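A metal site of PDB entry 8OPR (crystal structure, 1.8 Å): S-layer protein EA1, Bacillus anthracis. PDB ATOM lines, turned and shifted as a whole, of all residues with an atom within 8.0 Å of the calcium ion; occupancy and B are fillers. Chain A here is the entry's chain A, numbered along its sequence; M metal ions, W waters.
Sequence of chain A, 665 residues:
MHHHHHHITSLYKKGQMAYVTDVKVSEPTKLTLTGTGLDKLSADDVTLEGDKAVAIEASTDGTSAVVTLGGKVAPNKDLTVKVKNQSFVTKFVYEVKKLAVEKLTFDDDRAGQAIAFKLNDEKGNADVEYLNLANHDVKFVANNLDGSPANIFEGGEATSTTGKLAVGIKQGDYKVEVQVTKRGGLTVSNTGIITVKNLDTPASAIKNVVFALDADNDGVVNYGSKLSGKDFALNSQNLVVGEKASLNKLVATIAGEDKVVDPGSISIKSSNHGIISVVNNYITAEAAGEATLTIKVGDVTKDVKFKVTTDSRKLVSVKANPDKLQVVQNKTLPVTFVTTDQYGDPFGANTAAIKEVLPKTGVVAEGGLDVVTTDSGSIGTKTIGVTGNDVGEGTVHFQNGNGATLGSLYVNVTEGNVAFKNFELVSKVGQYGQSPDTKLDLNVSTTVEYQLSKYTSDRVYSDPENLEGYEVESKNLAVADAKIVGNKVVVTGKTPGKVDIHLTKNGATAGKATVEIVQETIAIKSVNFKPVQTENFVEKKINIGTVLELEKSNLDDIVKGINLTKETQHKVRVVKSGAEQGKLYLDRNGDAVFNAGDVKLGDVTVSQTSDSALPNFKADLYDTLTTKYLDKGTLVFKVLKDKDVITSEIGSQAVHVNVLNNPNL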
ATOM      1  N   ALA A 212       4.353  16.890  -8.046  1.00  0.00           N
ATOM      2  CA  ALA A 212       4.997  15.833  -7.307  1.00  0.00           C
ATOM      3  C   ALA A 212       4.672  14.506  -7.949  1.00  0.00           C
ATOM      4  O   ALA A 212       3.531  14.264  -8.317  1.00  0.00           O
ATOM      5  CB  ALA A 212       4.520  15.831  -5.856  1.00  0.00           C
ATOM      6  N   LEU A 213       5.682  13.639  -8.063  1.00  0.00           N
ATOM      7  CA  LEU A 213       5.501  12.309  -8.594  1.00  0.00           C
ATOM      8  C   LEU A 213       4.794  11.422  -7.577  1.00  0.00           C
ATOM      9  O   LEU A 213       5.221  11.360  -6.427  1.00  0.00           O
ATOM     10  CB  LEU A 213       6.890  11.674  -8.877  1.00  0.00           C
ATOM     11  CG  LEU A 213       6.871  10.580  -9.960  1.00  0.00           C
ATOM     12  CD1 LEU A 213       6.598  11.192 -11.327  1.00  0.00           C
ATOM     13  CD2 LEU A 213       8.152   9.836  -9.996  1.00  0.00           C
ATOM     14  N   ASP A 214       3.811  10.661  -8.007  1.00  0.00           N
ATOM     15  CA  ASP A 214       3.205   9.631  -7.180  1.00  0.00           C
ATOM     16  C   ASP A 214       4.149   8.448  -7.375  1.00  0.00           C
ATOM     17  O   ASP A 214       3.863   7.532  -8.175  1.00  0.00           O
ATOM     18  CB  ASP A 214       1.803   9.275  -7.692  1.00  0.00           C
ATOM     19  CG  ASP A 214       1.083   8.249  -6.823  1.00  0.00           C
ATOM     20  OD1 ASP A 214       1.539   8.020  -5.698  1.00  0.00           O
ATOM     21  OD2 ASP A 214       0.067   7.675  -7.291  1.00  0.00           O
ATOM     22  N   ALA A 215       5.312   8.518  -6.727  1.00  0.00           N
ATOM     23  CA  ALA A 215       6.393   7.568  -6.925  1.00  0.00           C
ATOM     24  C   ALA A 215       6.093   6.163  -6.459  1.00  0.00           C
ATOM     25  O   ALA A 215       6.687   5.239  -6.984  1.00  0.00           O
ATOM     26  CB  ALA A 215       7.661   8.071  -6.278  1.00  0.00           C
ATOM     27  N   ASP A 216       5.199   6.002  -5.484  1.00  0.00           N
ATOM     28  CA  ASP A 216       4.818   4.664  -5.038  1.00  0.00           C
ATOM     29  C   ASP A 216       3.516   4.172  -5.705  1.00  0.00           C
ATOM     30  O   ASP A 216       2.965   3.173  -5.262  1.00  0.00           O
ATOM     31  CB  ASP A 216       4.703   4.606  -3.512  1.00  0.00           C
ATOM     32  CG  ASP A 216       3.909   5.739  -2.905  1.00  0.00           C
ATOM     33  OD1 ASP A 216       3.022   6.280  -3.606  1.00  0.00           O
ATOM     34  OD2 ASP A 216       4.184   6.100  -1.747  1.00  0.00           O
ATOM     35  N   ASN A 217       3.012   4.886  -6.729  1.00  0.00           N
ATOM     36  CA  ASN A 217       1.820   4.542  -7.474  1.00  0.00           C
ATOM     37  C   ASN A 217       0.634   4.131  -6.547  1.00  0.00           C
ATOM     38  O   ASN A 217      -0.014   3.118  -6.795  1.00  0.00           O
ATOM     39  CB  ASN A 217       2.168   3.462  -8.510  1.00  0.00           C
ATOM     40  CG  ASN A 217       1.047   3.096  -9.443  1.00  0.00           C
ATOM     41  OD1 ASN A 217       0.189   3.907  -9.764  1.00  0.00           O
ATOM     42  ND2 ASN A 217       0.999   1.856  -9.865  1.00  0.00           N
ATOM     43  N   ASP A 218       0.363   4.893  -5.480  1.00  0.00           N
ATOM     44  CA  ASP A 218      -0.727   4.573  -4.558  1.00  0.00           C
ATOM     45  C   ASP A 218      -1.999   5.450  -4.748  1.00  0.00           C
ATOM     46  O   ASP A 218      -2.940   5.300  -3.976  1.00  0.00           O
ATOM     47  CB  ASP A 218      -0.248   4.590  -3.073  1.00  0.00           C
ATOM     48  CG  ASP A 218       0.109   5.939  -2.498  1.00  0.00           C
ATOM     49  OD1 ASP A 218       0.129   6.926  -3.259  1.00  0.00           O
ATOM     50  OD2 ASP A 218       0.412   6.008  -1.292  1.00  0.00           O
ATOM     51  N   GLY A 219      -1.994   6.336  -5.756  1.00  0.00           N
ATOM     52  CA  GLY A 219      -3.113   7.233  -6.014  1.00  0.00           C
ATOM     53  C   GLY A 219      -3.190   8.430  -5.068  1.00  0.00           C
ATOM     54  O   GLY A 219      -4.106   9.246  -5.193  1.00  0.00           O
ATOM     55  N   VAL A 220      -2.280   8.529  -4.107  1.00  0.00           N
ATOM     56  CA  VAL A 220      -2.277   9.626  -3.142  1.00  0.00           C
ATOM     57  C   VAL A 220      -1.074  10.518  -3.374  1.00  0.00           C
ATOM     58  O   VAL A 220       0.050  10.027  -3.304  1.00  0.00           O
ATOM     59  CB  VAL A 220      -2.204   9.081  -1.676  1.00  0.00           C
ATOM     60  CG1 VAL A 220      -2.359  10.204  -0.646  1.00  0.00           C
ATOM     61  CG2 VAL A 220      -3.252   8.004  -1.438  1.00  0.00           C
ATOM     62  N   VAL A 221      -1.292  11.838  -3.577  1.00  0.00           N
ATOM     63  CA  VAL A 221      -0.212  12.821  -3.670  1.00  0.00           C
ATOM     64  C   VAL A 221      -0.684  13.957  -2.812  1.00  0.00           C
ATOM     65  O   VAL A 221      -1.644  14.649  -3.182  1.00  0.00           O
ATOM     66  CB  VAL A 221       0.136  13.326  -5.095  1.00  0.00           C
ATOM     67  CG1 VAL A 221       1.180  14.437  -5.041  1.00  0.00           C
ATOM     68  CG2 VAL A 221       0.618  12.193  -6.007  1.00  0.00           C
ATOM     69  N   ASN A 222      -0.028  14.157  -1.636  1.00  0.00           N
ATOM     70  CA  ASN A 222      -0.440  15.233  -0.749  1.00  0.00           C
ATOM     71  C   ASN A 222      -0.256  16.591  -1.364  1.00  0.00           C
ATOM     72  O   ASN A 222       0.743  16.869  -2.037  1.00  0.00           O
ATOM     73  CB  ASN A 222       0.319  15.184   0.588  1.00  0.00           C
ATOM     74  CG  ASN A 222       0.010  13.949   1.389  1.00  0.00           C
ATOM     75  OD1 ASN A 222      -1.015  13.291   1.203  1.00  0.00           O
ATOM     76  ND2 ASN A 222       0.905  13.615   2.279  1.00  0.00           N
ATOM     77  N   LEU A 227       4.857  15.509   1.576  1.00  0.00           N
ATOM     78  CA  LEU A 227       4.572  14.318   0.814  1.00  0.00           C
ATOM     79  C   LEU A 227       4.756  13.058   1.668  1.00  0.00           C
ATOM     80  O   LEU A 227       5.420  13.106   2.698  1.00  0.00           O
ATOM     81  CB  LEU A 227       5.464  14.300  -0.430  1.00  0.00           C
ATOM     82  CG  LEU A 227       5.080  15.392  -1.410  1.00  0.00           C
ATOM     83  CD1 LEU A 227       6.162  15.660  -2.383  1.00  0.00           C
ATOM     84  CD2 LEU A 227       3.758  15.073  -2.089  1.00  0.00           C
ATOM     85  N   SER A 228       4.162  11.964   1.265  1.00  0.00           N
ATOM     86  CA  SER A 228       4.187  10.718   2.028  1.00  0.00           C
ATOM     87  C   SER A 228       4.703   9.577   1.155  1.00  0.00           C
ATOM     88  O   SER A 228       4.684   9.669  -0.072  1.00  0.00           O
ATOM     89  CB  SER A 228       2.777  10.406   2.539  1.00  0.00           C
ATOM     90  OG  SER A 228       1.817  10.377   1.483  1.00  0.00           O
ATOM     91  N   GLY A 229       5.139   8.504   1.777  1.00  0.00           N
ATOM     92  CA  GLY A 229       5.669   7.357   1.051  1.00  0.00           C
ATOM     93  C   GLY A 229       6.931   7.722   0.280  1.00  0.00           C
ATOM     94  O   GLY A 229       7.790   8.462   0.780  1.00  0.00           O
ATOM     95  N   LYS A 230       6.984   7.277  -0.992  1.00  0.00           N
ATOM     96  CA  LYS A 230       8.098   7.524  -1.902  1.00  0.00           C
ATOM     97  C   LYS A 230       7.942   8.831  -2.715  1.00  0.00           C
ATOM     98  O   LYS A 230       8.869   9.203  -3.418  1.00  0.00           O
ATOM     99  CB  LYS A 230       8.233   6.340  -2.853  1.00  0.00           C
ATOM    100  CG  LYS A 230       8.391   5.023  -2.108  1.00  0.00           C
ATOM    101  CD  LYS A 230       8.769   3.910  -3.056  1.00  0.00           C
ATOM    102  CE  LYS A 230       9.794   2.987  -2.447  1.00  0.00           C
ATOM    103  NZ  LYS A 230      10.405   2.093  -3.485  1.00  0.00           N
ATOM    104  N   ASP A 231       6.805   9.525  -2.607  1.00  0.00           N
ATOM    105  CA  ASP A 231       6.529  10.751  -3.341  1.00  0.00           C
ATOM    106  C   ASP A 231       7.531  11.865  -3.154  1.00  0.00           C
ATOM    107  O   ASP A 231       8.023  12.112  -2.045  1.00  0.00           O
ATOM    108  CB  ASP A 231       5.114  11.287  -3.037  1.00  0.00           C
ATOM    109  CG  ASP A 231       3.996  10.316  -3.351  1.00  0.00           C
ATOM    110  OD1 ASP A 231       4.298   9.199  -3.880  1.00  0.00           O
ATOM    111  OD2 ASP A 231       2.842  10.646  -3.068  1.00  0.00           O
ATOM    112  N   PHE A 232       7.837  12.562  -4.243  1.00  0.00           N
ATOM    113  CA  PHE A 232       8.789  13.663  -4.208  1.00  0.00           C
ATOM    114  C   PHE A 232       8.339  14.781  -5.125  1.00  0.00           C
ATOM    115  O   PHE A 232       7.652  14.540  -6.125  1.00  0.00           O
ATOM    116  CB  PHE A 232      10.222  13.198  -4.523  1.00  0.00           C
ATOM    117  CG  PHE A 232      10.429  12.503  -5.837  1.00  0.00           C
ATOM    118  CD1 PHE A 232      10.689  13.231  -6.986  1.00  0.00           C
ATOM    119  CD2 PHE A 232      10.410  11.129  -5.921  1.00  0.00           C
ATOM    120  CE1 PHE A 232      10.914  12.599  -8.180  1.00  0.00           C
ATOM    121  CE2 PHE A 232      10.629  10.501  -7.123  1.00  0.00           C
ATOM    122  CZ  PHE A 232      10.874  11.232  -8.255  1.00  0.00           C
ATOM    123  N   LYS A 244       2.971   8.740 -12.857  1.00  0.00           N
ATOM    124  CA  LYS A 244       1.812   9.534 -12.497  1.00  0.00           C
ATOM    125  C   LYS A 244       2.279  10.663 -11.572  1.00  0.00           C
ATOM    126  O   LYS A 244       3.237  10.499 -10.824  1.00  0.00           O
ATOM    127  CB  LYS A 244       0.760   8.672 -11.814  1.00  0.00           C
ATOM    128  CG  LYS A 244       0.076   7.713 -12.780  1.00  0.00           C
ATOM    129  CD  LYS A 244       0.199   6.331 -12.243  1.00  0.00           C
ATOM    130  CE  LYS A 244      -0.488   5.297 -13.080  1.00  0.00           C
ATOM    131  NZ  LYS A 244      -1.192   4.318 -12.218  1.00  0.00           N
ATOM    132  N   TYR A 282      -4.865  14.856 -11.509  1.00  0.00           N
ATOM    133  CA  TYR A 282      -3.904  13.757 -11.377  1.00  0.00           C
ATOM    134  C   TYR A 282      -3.494  13.382 -12.805  1.00  0.00           C
ATOM    135  O   TYR A 282      -4.364  13.046 -13.627  1.00  0.00           O
ATOM    136  CB  TYR A 282      -4.540  12.591 -10.634  1.00  0.00           C
ATOM    137  CG  TYR A 282      -3.632  11.431 -10.331  1.00  0.00           C
ATOM    138  CD1 TYR A 282      -2.872  11.391  -9.172  1.00  0.00           C
ATOM    139  CD2 TYR A 282      -3.637  10.289 -11.137  1.00  0.00           C
ATOM    140  CE1 TYR A 282      -2.134  10.280  -8.824  1.00  0.00           C
ATOM    141  CE2 TYR A 282      -2.877   9.178 -10.812  1.00  0.00           C
ATOM    142  CZ  TYR A 282      -2.129   9.171  -9.652  1.00  0.00           C
ATOM    143  OH  TYR A 282      -1.420   8.052  -9.311  1.00  0.00           O
HETATM  144 CA    CA M   1       1.857   8.515  -3.477  1.00  0.00          CA
HETATM  145  O   HOH W   1       2.573   8.084  -1.092  1.00  0.00           O
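Of the 19 residues printed, 5 come within 4 Å of the calcium ion.
OD1 of Asp 214 is bound to the calcium ion, at 2.3 Å. OD1 of Asp 218 is bound to the calcium ion, at 2.4 Å. The calcium ion is bound by the backbone carbonyl oxygen (O) of Val 220, 2.4 Å away. The side-chain carboxylate (OD2) of Asp 231 is bound to the calcium ion (2.4 Å). OD1 of Asp 216 binds the calcium ion (2.5 Å). The calcium ion is bound by water W1 (2.5 Å). The calcium ion is bound by OD1 of Asp 231 (2.6 Å).
OD2 of Asp 216 sits at hydrogen-bond distance from N of Lys 230 (3.1 Å). OD1 of Asp 231 sits close to N of Ala 215, at 3.1 Å. OD2 of Asp 214 sits at hydrogen-bond distance from N of Gly 219, 2.9 Å away. N of Asp 214 is in hydrogen-bond range of O of Lys 244, at 2.9 Å. The side-chain hydroxyl (OH) of Tyr 282 sits at hydrogen-bond distance from the side-chain carboxylate (OD2) of Asp 214, 2.5 Å away.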
